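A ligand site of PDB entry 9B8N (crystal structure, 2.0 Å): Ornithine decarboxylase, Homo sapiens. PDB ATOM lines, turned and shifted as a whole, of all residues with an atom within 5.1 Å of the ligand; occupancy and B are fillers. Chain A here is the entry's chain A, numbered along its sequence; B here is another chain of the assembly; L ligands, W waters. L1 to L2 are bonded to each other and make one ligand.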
ATOM      1  N   ALA A  67      33.048 -16.782 -15.024  1.00  0.00           N
ATOM      2  CA  ALA A  67      32.262 -15.558 -15.186  1.00  0.00           C
ATOM      3  C   ALA A  67      33.225 -14.372 -15.237  1.00  0.00           C
ATOM      4  O   ALA A  67      33.656 -13.854 -14.205  1.00  0.00           O
ATOM      5  CB  ALA A  67      31.259 -15.418 -14.039  1.00  0.00           C
ATOM      6  N   LYS A  69      32.956 -11.319 -15.768  1.00  0.00           N
ATOM      7  CA  LYS A  69      32.550 -10.075 -15.119  1.00  0.00           C
ATOM      8  C   LYS A  69      33.041  -9.981 -13.686  1.00  0.00           C
ATOM      9  O   LYS A  69      33.191  -8.878 -13.147  1.00  0.00           O
ATOM     10  CB  LYS A  69      31.031  -9.953 -15.141  1.00  0.00           C
ATOM     11  CG  LYS A  69      30.341 -11.071 -14.393  1.00  0.00           C
ATOM     12  CD  LYS A  69      28.850 -10.852 -14.313  1.00  0.00           C
ATOM     13  CE  LYS A  69      28.068 -12.149 -14.418  1.00  0.00           C
ATOM     14  NZ  LYS A  69      28.224 -12.804 -15.745  1.00  0.00           N
ATOM     15  N   CYS A  70      33.271 -11.127 -13.033  1.00  0.00           N
ATOM     16  CA  CYS A  70      33.687 -11.115 -11.633  1.00  0.00           C
ATOM     17  C   CYS A  70      35.059 -10.466 -11.476  1.00  0.00           C
ATOM     18  O   CYS A  70      35.290  -9.697 -10.533  1.00  0.00           O
ATOM     19  CB  CYS A  70      33.691 -12.544 -11.096  1.00  0.00           C
ATOM     20  SG  CYS A  70      34.241 -12.691  -9.402  1.00  0.00           S
ATOM     21  N   ASP A  88      32.000 -17.493 -19.388  1.00  0.00           N
ATOM     22  CA  ASP A  88      30.696 -16.859 -19.414  1.00  0.00           C
ATOM     23  C   ASP A  88      30.908 -15.371 -19.627  1.00  0.00           C
ATOM     24  O   ASP A  88      31.488 -14.691 -18.768  1.00  0.00           O
ATOM     25  CB  ASP A  88      29.943 -17.155 -18.109  1.00  0.00           C
ATOM     26  CG  ASP A  88      28.855 -16.134 -17.798  1.00  0.00           C
ATOM     27  OD1 ASP A  88      28.308 -15.506 -18.725  1.00  0.00           O
ATOM     28  OD2 ASP A  88      28.553 -15.954 -16.599  1.00  0.00           O
ATOM     29  N   ALA A 111      25.996 -15.500 -21.574  1.00  0.00           N
ATOM     30  CA  ALA A 111      24.982 -15.769 -20.560  1.00  0.00           C
ATOM     31  C   ALA A 111      24.388 -14.491 -19.968  1.00  0.00           C
ATOM     32  O   ALA A 111      24.266 -14.334 -18.760  1.00  0.00           O
ATOM     33  CB  ALA A 111      25.562 -16.656 -19.465  1.00  0.00           C
ATOM     34  N   ARG A 154      16.843 -19.540 -19.228  1.00  0.00           N
ATOM     35  CA  ARG A 154      17.192 -19.283 -17.840  1.00  0.00           C
ATOM     36  C   ARG A 154      15.929 -19.232 -16.988  1.00  0.00           C
ATOM     37  O   ARG A 154      15.018 -18.436 -17.264  1.00  0.00           O
ATOM     38  CB  ARG A 154      17.971 -17.987 -17.689  1.00  0.00           C
ATOM     39  CG  ARG A 154      18.325 -17.711 -16.244  1.00  0.00           C
ATOM     40  CD  ARG A 154      19.421 -16.687 -16.106  1.00  0.00           C
ATOM     41  NE  ARG A 154      19.543 -16.223 -14.723  1.00  0.00           N
ATOM     42  CZ  ARG A 154      20.308 -15.208 -14.354  1.00  0.00           C
ATOM     43  NH1 ARG A 154      21.015 -14.559 -15.260  1.00  0.00           N
ATOM     44  NH2 ARG A 154      20.367 -14.850 -13.081  1.00  0.00           N
ATOM     45  N   CYS A 164      23.267 -11.973  -2.724  1.00  0.00           N
ATOM     46  CA  CYS A 164      23.008 -11.139  -3.898  1.00  0.00           C
ATOM     47  C   CYS A 164      21.892 -11.790  -4.713  1.00  0.00           C
ATOM     48  O   CYS A 164      22.121 -12.790  -5.403  1.00  0.00           O
ATOM     49  CB  CYS A 164      24.278 -10.971  -4.729  1.00  0.00           C
ATOM     50  SG  CYS A 164      25.656 -10.203  -3.844  1.00  0.00           S
ATOM     51  N   LEU A 166      19.318 -12.389  -7.638  1.00  0.00           N
ATOM     52  CA  LEU A 166      19.235 -12.162  -9.075  1.00  0.00           C
ATOM     53  C   LEU A 166      17.859 -12.460  -9.659  1.00  0.00           C
ATOM     54  O   LEU A 166      17.541 -11.953 -10.736  1.00  0.00           O
ATOM     55  CB  LEU A 166      20.268 -13.038  -9.800  1.00  0.00           C
ATOM     56  CG  LEU A 166      21.722 -12.907  -9.341  1.00  0.00           C
ATOM     57  CD1 LEU A 166      22.633 -13.797 -10.187  1.00  0.00           C
ATOM     58  CD2 LEU A 166      22.192 -11.458  -9.395  1.00  0.00           C
ATOM     59  N   HIS A 197      20.568 -19.557 -11.785  1.00  0.00           N
ATOM     60  CA  HIS A 197      21.572 -19.012 -10.875  1.00  0.00           C
ATOM     61  C   HIS A 197      20.932 -18.903  -9.490  1.00  0.00           C
ATOM     62  O   HIS A 197      19.968 -18.160  -9.309  1.00  0.00           O
ATOM     63  CB  HIS A 197      22.099 -17.659 -11.350  1.00  0.00           C
ATOM     64  CG  HIS A 197      23.370 -17.244 -10.680  1.00  0.00           C
ATOM     65  ND1 HIS A 197      23.454 -16.993  -9.328  1.00  0.00           N
ATOM     66  CD2 HIS A 197      24.627 -17.077 -11.167  1.00  0.00           C
ATOM     67  CE1 HIS A 197      24.695 -16.671  -9.012  1.00  0.00           C
ATOM     68  NE2 HIS A 197      25.423 -16.713 -10.110  1.00  0.00           N
ATOM     69  N   GLY A 199      22.037 -17.518  -6.958  1.00  0.00           N
ATOM     70  CA  GLY A 199      22.319 -16.215  -6.388  1.00  0.00           C
ATOM     71  C   GLY A 199      23.727 -16.205  -5.849  1.00  0.00           C
ATOM     72  O   GLY A 199      24.207 -17.193  -5.272  1.00  0.00           O
ATOM     73  N   SER A 200      24.415 -15.091  -6.042  1.00  0.00           N
ATOM     74  CA  SER A 200      25.783 -14.974  -5.548  1.00  0.00           C
ATOM     75  C   SER A 200      25.786 -15.002  -4.026  1.00  0.00           C
ATOM     76  O   SER A 200      24.916 -14.416  -3.386  1.00  0.00           O
ATOM     77  CB  SER A 200      26.427 -13.695  -6.074  1.00  0.00           C
ATOM     78  OG  SER A 200      27.837 -13.831  -6.142  1.00  0.00           O
ATOM     79  N   GLY A 201      26.768 -15.682  -3.453  1.00  0.00           N
ATOM     80  CA  GLY A 201      26.776 -15.820  -2.011  1.00  0.00           C
ATOM     81  C   GLY A 201      25.652 -16.695  -1.498  1.00  0.00           C
ATOM     82  O   GLY A 201      24.858 -16.259  -0.663  1.00  0.00           O
ATOM     83  N   GLY A 236      26.297 -19.968 -10.863  1.00  0.00           N
ATOM     84  CA  GLY A 236      27.349 -19.682  -9.906  1.00  0.00           C
ATOM     85  C   GLY A 236      26.856 -19.642  -8.470  1.00  0.00           C
ATOM     86  O   GLY A 236      25.938 -20.372  -8.105  1.00  0.00           O
ATOM     87  N   GLY A 237      27.472 -18.793  -7.657  1.00  0.00           N
ATOM     88  CA  GLY A 237      27.120 -18.656  -6.259  1.00  0.00           C
ATOM     89  C   GLY A 237      28.011 -19.379  -5.275  1.00  0.00           C
ATOM     90  O   GLY A 237      27.799 -19.268  -4.065  1.00  0.00           O
ATOM     91  N   PHE A 238      29.008 -20.122  -5.762  1.00  0.00           N
ATOM     92  CA  PHE A 238      29.911 -20.844  -4.883  1.00  0.00           C
ATOM     93  C   PHE A 238      30.844 -19.880  -4.152  1.00  0.00           C
ATOM     94  O   PHE A 238      31.247 -18.857  -4.700  1.00  0.00           O
ATOM     95  CB  PHE A 238      30.725 -21.854  -5.683  1.00  0.00           C
ATOM     96  CG  PHE A 238      29.888 -22.718  -6.598  1.00  0.00           C
ATOM     97  CD1 PHE A 238      29.293 -23.868  -6.124  1.00  0.00           C
ATOM     98  CD2 PHE A 238      29.693 -22.355  -7.921  1.00  0.00           C
ATOM     99  CE1 PHE A 238      28.516 -24.657  -6.959  1.00  0.00           C
ATOM    100  CE2 PHE A 238      28.922 -23.139  -8.763  1.00  0.00           C
ATOM    101  CZ  PHE A 238      28.328 -24.295  -8.276  1.00  0.00           C
ATOM    102  N   GLU A 274      28.783 -21.617 -14.100  1.00  0.00           N
ATOM    103  CA  GLU A 274      29.299 -20.269 -14.354  1.00  0.00           C
ATOM    104  C   GLU A 274      29.922 -19.675 -13.090  1.00  0.00           C
ATOM    105  O   GLU A 274      29.523 -18.591 -12.649  1.00  0.00           O
ATOM    106  CB  GLU A 274      28.193 -19.362 -14.878  1.00  0.00           C
ATOM    107  CG  GLU A 274      27.475 -19.833 -16.125  1.00  0.00           C
ATOM    108  CD  GLU A 274      26.149 -19.130 -16.314  1.00  0.00           C
ATOM    109  OE1 GLU A 274      25.661 -18.492 -15.356  1.00  0.00           O
ATOM    110  OE2 GLU A 274      25.595 -19.180 -17.431  1.00  0.00           O
ATOM    111  N   PRO A 275      30.892 -20.349 -12.473  1.00  0.00           N
ATOM    112  CA  PRO A 275      31.461 -19.811 -11.231  1.00  0.00           C
ATOM    113  C   PRO A 275      32.268 -18.548 -11.505  1.00  0.00           C
ATOM    114  O   PRO A 275      33.135 -18.532 -12.374  1.00  0.00           O
ATOM    115  CB  PRO A 275      32.350 -20.957 -10.723  1.00  0.00           C
ATOM    116  CG  PRO A 275      32.788 -21.643 -11.978  1.00  0.00           C
ATOM    117  CD  PRO A 275      31.618 -21.555 -12.932  1.00  0.00           C
ATOM    118  N   GLY A 276      31.945 -17.473 -10.775  1.00  0.00           N
ATOM    119  CA  GLY A 276      32.839 -16.334 -10.787  1.00  0.00           C
ATOM    120  C   GLY A 276      33.735 -16.165  -9.569  1.00  0.00           C
ATOM    121  O   GLY A 276      34.957 -16.309  -9.684  1.00  0.00           O
ATOM    122  N   ARG A 277      33.151 -15.921  -8.393  1.00  0.00           N
ATOM    123  CA  ARG A 277      33.989 -15.587  -7.252  1.00  0.00           C
ATOM    124  C   ARG A 277      34.779 -16.793  -6.748  1.00  0.00           C
ATOM    125  O   ARG A 277      35.847 -16.604  -6.152  1.00  0.00           O
ATOM    126  CB  ARG A 277      33.169 -14.970  -6.108  1.00  0.00           C
ATOM    127  CG  ARG A 277      32.373 -15.924  -5.250  1.00  0.00           C
ATOM    128  CD  ARG A 277      31.728 -15.188  -4.074  1.00  0.00           C
ATOM    129  NE  ARG A 277      30.598 -14.344  -4.476  1.00  0.00           N
ATOM    130  CZ  ARG A 277      30.547 -13.025  -4.314  1.00  0.00           C
ATOM    131  NH1 ARG A 277      29.472 -12.344  -4.709  1.00  0.00           N
ATOM    132  NH2 ARG A 277      31.561 -12.385  -3.748  1.00  0.00           N
ATOM    133  N   TYR A 278      34.286 -18.012  -6.997  1.00  0.00           N
ATOM    134  CA  TYR A 278      34.979 -19.211  -6.549  1.00  0.00           C
ATOM    135  C   TYR A 278      36.424 -19.243  -7.047  1.00  0.00           C
ATOM    136  O   TYR A 278      37.340 -19.624  -6.300  1.00  0.00           O
ATOM    137  CB  TYR A 278      34.241 -20.465  -7.011  1.00  0.00           C
ATOM    138  CG  TYR A 278      35.082 -21.717  -6.869  1.00  0.00           C
ATOM    139  CD1 TYR A 278      35.174 -22.372  -5.650  1.00  0.00           C
ATOM    140  CD2 TYR A 278      35.790 -22.231  -7.949  1.00  0.00           C
ATOM    141  CE1 TYR A 278      35.959 -23.503  -5.505  1.00  0.00           C
ATOM    142  CE2 TYR A 278      36.567 -23.361  -7.811  1.00  0.00           C
ATOM    143  CZ  TYR A 278      36.651 -23.994  -6.595  1.00  0.00           C
ATOM    144  OH  TYR A 278      37.429 -25.124  -6.457  1.00  0.00           O
ATOM    145  N   TYR A 331      28.083  -2.587  -3.579  1.00  0.00           N
ATOM    146  CA  TYR A 331      27.496  -3.415  -4.631  1.00  0.00           C
ATOM    147  C   TYR A 331      27.421  -4.894  -4.254  1.00  0.00           C
ATOM    148  O   TYR A 331      26.480  -5.583  -4.639  1.00  0.00           O
ATOM    149  CB  TYR A 331      28.275  -3.241  -5.937  1.00  0.00           C
ATOM    150  CG  TYR A 331      28.109  -1.889  -6.573  1.00  0.00           C
ATOM    151  CD1 TYR A 331      26.943  -1.550  -7.258  1.00  0.00           C
ATOM    152  CD2 TYR A 331      29.115  -0.940  -6.511  1.00  0.00           C
ATOM    153  CE1 TYR A 331      26.797  -0.308  -7.856  1.00  0.00           C
ATOM    154  CE2 TYR A 331      28.984   0.301  -7.096  1.00  0.00           C
ATOM    155  CZ  TYR A 331      27.816   0.619  -7.767  1.00  0.00           C
ATOM    156  OH  TYR A 331      27.688   1.852  -8.356  1.00  0.00           O
ATOM    157  N   ASP A 332      28.418  -5.403  -3.525  1.00  0.00           N
ATOM    158  CA  ASP A 332      28.531  -6.840  -3.275  1.00  0.00           C
ATOM    159  C   ASP A 332      28.226  -7.224  -1.835  1.00  0.00           C
ATOM    160  O   ASP A 332      28.432  -8.384  -1.456  1.00  0.00           O
ATOM    161  CB  ASP A 332      29.936  -7.326  -3.671  1.00  0.00           C
ATOM    162  CG  ASP A 332      29.994  -8.831  -3.880  1.00  0.00           C
ATOM    163  OD1 ASP A 332      30.993  -9.450  -3.453  1.00  0.00           O
ATOM    164  OD2 ASP A 332      29.037  -9.398  -4.456  1.00  0.00           O
ATOM    165  N   TYR A 389      34.644  -9.099  -7.635  1.00  0.00           N
ATOM    166  CA  TYR A 389      33.768  -7.917  -7.673  1.00  0.00           C
ATOM    167  C   TYR A 389      34.389  -6.741  -6.927  1.00  0.00           C
ATOM    168  O   TYR A 389      33.706  -5.992  -6.217  1.00  0.00           O
ATOM    169  CB  TYR A 389      32.387  -8.256  -7.131  1.00  0.00           C
ATOM    170  CG  TYR A 389      31.756  -9.433  -7.837  1.00  0.00           C
ATOM    171  CD1 TYR A 389      31.304  -9.312  -9.133  1.00  0.00           C
ATOM    172  CD2 TYR A 389      31.644 -10.670  -7.206  1.00  0.00           C
ATOM    173  CE1 TYR A 389      30.749 -10.385  -9.803  1.00  0.00           C
ATOM    174  CE2 TYR A 389      31.083 -11.748  -7.870  1.00  0.00           C
ATOM    175  CZ  TYR A 389      30.637 -11.599  -9.169  1.00  0.00           C
ATOM    176  OH  TYR A 389      30.086 -12.665  -9.827  1.00  0.00           O
ATOM    177  N   TYR B 323      25.996   0.755 -12.253  1.00  0.00           N
ATOM    178  CA  TYR B 323      27.452   0.709 -12.345  1.00  0.00           C
ATOM    179  C   TYR B 323      27.990   1.775 -13.276  1.00  0.00           C
ATOM    180  O   TYR B 323      29.181   2.089 -13.220  1.00  0.00           O
ATOM    181  CB  TYR B 323      27.915  -0.673 -12.791  1.00  0.00           C
ATOM    182  CG  TYR B 323      27.706  -1.756 -11.762  1.00  0.00           C
ATOM    183  CD1 TYR B 323      26.521  -2.482 -11.716  1.00  0.00           C
ATOM    184  CD2 TYR B 323      28.695  -2.055 -10.830  1.00  0.00           C
ATOM    185  CE1 TYR B 323      26.328  -3.467 -10.766  1.00  0.00           C
ATOM    186  CE2 TYR B 323      28.513  -3.049  -9.878  1.00  0.00           C
ATOM    187  CZ  TYR B 323      27.319  -3.746  -9.848  1.00  0.00           C
ATOM    188  OH  TYR B 323      27.128  -4.733  -8.916  1.00  0.00           O
ATOM    189  N   CYS B 360      24.252  -7.840 -14.847  1.00  0.00           N
ATOM    190  CA  CYS B 360      23.731  -9.040 -14.207  1.00  0.00           C
ATOM    191  C   CYS B 360      23.161  -8.786 -12.821  1.00  0.00           C
ATOM    192  O   CYS B 360      22.398  -9.621 -12.313  1.00  0.00           O
ATOM    193  CB  CYS B 360      24.845 -10.059 -14.067  1.00  0.00           C
ATOM    194  SG  CYS B 360      26.179  -9.410 -13.014  1.00  0.00           S
ATOM    195  N   ASP B 361      23.518  -7.674 -12.181  1.00  0.00           N
ATOM    196  CA  ASP B 361      23.165  -7.464 -10.786  1.00  0.00           C
ATOM    197  C   ASP B 361      21.664  -7.272 -10.639  1.00  0.00           C
ATOM    198  O   ASP B 361      21.063  -6.402 -11.279  1.00  0.00           O
ATOM    199  CB  ASP B 361      23.921  -6.255 -10.229  1.00  0.00           C
ATOM    200  CG  ASP B 361      23.774  -6.100  -8.726  1.00  0.00           C
ATOM    201  OD1 ASP B 361      22.926  -6.792  -8.120  1.00  0.00           O
ATOM    202  OD2 ASP B 361      24.514  -5.270  -8.144  1.00  0.00           O
ATOM    203  N   PHE B 397      31.951  -2.222 -15.230  1.00  0.00           N
ATOM    204  CA  PHE B 397      31.501  -3.535 -14.775  1.00  0.00           C
ATOM    205  C   PHE B 397      30.656  -4.189 -15.861  1.00  0.00           C
ATOM    206  O   PHE B 397      29.866  -3.529 -16.529  1.00  0.00           O
ATOM    207  CB  PHE B 397      30.708  -3.402 -13.472  1.00  0.00           C
ATOM    208  CG  PHE B 397      30.268  -4.719 -12.893  1.00  0.00           C
ATOM    209  CD1 PHE B 397      31.201  -5.668 -12.497  1.00  0.00           C
ATOM    210  CD2 PHE B 397      28.925  -5.000 -12.716  1.00  0.00           C
ATOM    211  CE1 PHE B 397      30.802  -6.881 -11.950  1.00  0.00           C
ATOM    212  CE2 PHE B 397      28.523  -6.205 -12.164  1.00  0.00           C
ATOM    213  CZ  PHE B 397      29.461  -7.142 -11.787  1.00  0.00           C
HETATM  214  N1  LIG L   1      26.545 -16.174 -13.936  1.00  0.00           N
HETATM  215  C1  LIG L   1      25.565 -15.198 -13.930  1.00  0.00           C
HETATM  216  C2  LIG L   1      24.479 -15.237 -14.966  1.00  0.00           C
HETATM  217  C3  LIG L   1      25.606 -14.205 -12.956  1.00  0.00           C
HETATM  218  O1  LIG L   1      24.634 -13.236 -12.931  1.00  0.00           O
HETATM  219  C4  LIG L   1      26.629 -14.188 -11.989  1.00  0.00           C
HETATM  220  C5  LIG L   1      26.597 -13.074 -10.978  1.00  0.00           C
HETATM  221  C6  LIG L   1      27.602 -15.180 -12.034  1.00  0.00           C
HETATM  222  C7  LIG L   1      27.550 -16.164 -13.010  1.00  0.00           C
HETATM  223  C8  LIG L   1      28.748 -15.284 -11.069  1.00  0.00           C
HETATM  224  O2  LIG L   1      28.275 -15.523  -9.767  1.00  0.00           O
HETATM  225  P1  LIG L   1      29.349 -15.908  -8.642  1.00  0.00           P
HETATM  226  O3  LIG L   1      28.607 -15.815  -7.341  1.00  0.00           O
HETATM  227  O4  LIG L   1      30.447 -14.898  -8.718  1.00  0.00           O
HETATM  228  O5  LIG L   1      29.876 -17.282  -8.949  1.00  0.00           O
HETATM  229  C1  LG2 L   2      26.785  -7.960  -7.011  1.00  0.00           C
HETATM  230  C2  LG2 L   2      28.014  -9.859  -7.462  1.00  0.00           C
HETATM  231  C3  LG2 L   2      26.039  -8.730  -8.103  1.00  0.00           C
HETATM  232  C4  LG2 L   2      27.028  -9.755  -8.604  1.00  0.00           C
HETATM  233  C5  LG2 L   2      26.396 -11.121  -8.943  1.00  0.00           C
HETATM  234  N1  LG2 L   2      28.151  -8.500  -6.919  1.00  0.00           N
HETATM  235  N2  LG2 L   2      25.805 -12.065 -11.191  1.00  0.00           N
HETATM  236  O1  LG2 L   2      25.634 -11.009 -10.257  1.00  0.00           O
HETATM  237  O   HOH W   1      31.415 -18.786  -7.501  1.00  0.00           O
HETATM  238  O   HOH W   2      22.358 -12.530 -13.505  1.00  0.00           O
HETATM  239  O   HOH W   3      29.085 -16.518  -5.028  1.00  0.00           O
HETATM  240  O   HOH W   4      29.329  -6.075  -7.732  1.00  0.00           O
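The side-chain hydroxyl of Ser 200 sits at hydrogen-bond distance from an oxygen (O3) of LIG L1 (2.4 Å).
The side-chain hydroxyl (OH) of Tyr 389 sits at hydrogen-bond distance from an oxygen (O4) of LIG L1 (2.5 Å).
The backbone NH (N) of Gly 276 lies within hydrogen-bond range of an oxygen (O5) of LIG L1.
The side-chain carboxylate of Asp 332 lies within salt-bridge range of a nitrogen (N1) of LG2 L2 (2.8 Å).
The side-chain carboxylate (OE1) of Glu 274 sits at hydrogen-bond distance from a nitrogen (N1) of LIG L1 (2.9 Å).
N of Arg 277 sits at hydrogen-bond distance from O4 of LIG L1 (2.9 Å).
NE of Arg 277 is in salt-bridge range of O3 of LIG L1.
An oxygen (O2) of LIG L1 is in hydrogen-bond range of a ring nitrogen (NE2) of His 197.
N of Gly 237 sits at hydrogen-bond distance from O5 of LIG L1 (3.1 Å).
SG of Cys 360 of chain B is in hydrogen-bond range of O1 of LG2 L2.
N of Tyr 389 is in hydrogen-bond range of O of Cys 70 (3.0 Å).
The backbone carbonyl oxygen of Gly 276 lies close to the side-chain sulfur of Cys 70, at 3.7 Å.
The side-chain carboxylate (OD2) of Asp 332 is in salt-bridge range of the guanidinium group (NH1) of Arg 277 (3.0 Å).
The side-chain carboxylate (OD2) of Asp 332 lies within hydrogen-bond range of the side-chain sulfur (SG) of Cys 164 (3.5 Å).
The backbone NH (N) of Arg 277 sits at hydrogen-bond distance from the side-chain sulfur (SG) of Cys 70 (3.6 Å).
The side-chain carboxylate (OD2) of Asp 88 is in salt-bridge range of the side-chain amino group (NZ) of Lys 69 (3.3 Å).
The side-chain carboxylate (OD2) of Asp 361 of chain B lies within hydrogen-bond range of the side-chain hydroxyl (OH) of Tyr 323 of chain B, 2.8 Å away.
The backbone NH of Ala 67 sits at hydrogen-bond distance from the backbone carbonyl oxygen of Pro 275 (3.2 Å).
OD2 of Asp 88 lies close to N1 of LIG L1, 3.3 Å away.
Merely in contact with the ligand: Ala 67, Lys 69, Ala 111, Arg 154, Leu 166, Gly 236, Pro 275, Tyr 331, Tyr 323 of chain B and Asp 361 of chain B.
Hydrophobic or aromatic side chains that line the ligand: Ala 67, Leu 166, His 197 and Tyr 389.
Water W2 lies within hydrogen-bond range of O1 of LIG L1 (2.5 Å), NH1 of Arg 154 (3.0 Å) and O of Cys 360 of chain B (3.1 Å).
Water W3 lies within hydrogen-bond range of an oxygen (O3) of LIG L1 (2.5 Å), the guanidinium group (NE) of Arg 277 (2.7 Å), the backbone NH (N) of Gly 201 (2.9 Å), the side-chain hydroxyl (OG) of Ser 200 (3.2 Å), the backbone carbonyl oxygen (O) of Gly 237 (3.2 Å) and the backbone carbonyl oxygen (O) of Phe 238 (3.2 Å).
Water W1 lies within hydrogen-bond range of an oxygen (O5) of LIG L1 (2.6 Å), the backbone carbonyl oxygen of Phe 238 (2.8 Å), the backbone NH of Tyr 278 (3.0 Å) and the backbone NH of Arg 277 (3.5 Å).
Water W4 bridges a nitrogen (N1) of LG2 L2 (2.8 Å) and the side-chain hydroxyl (OH) of Tyr 323 of chain B (2.8 Å).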
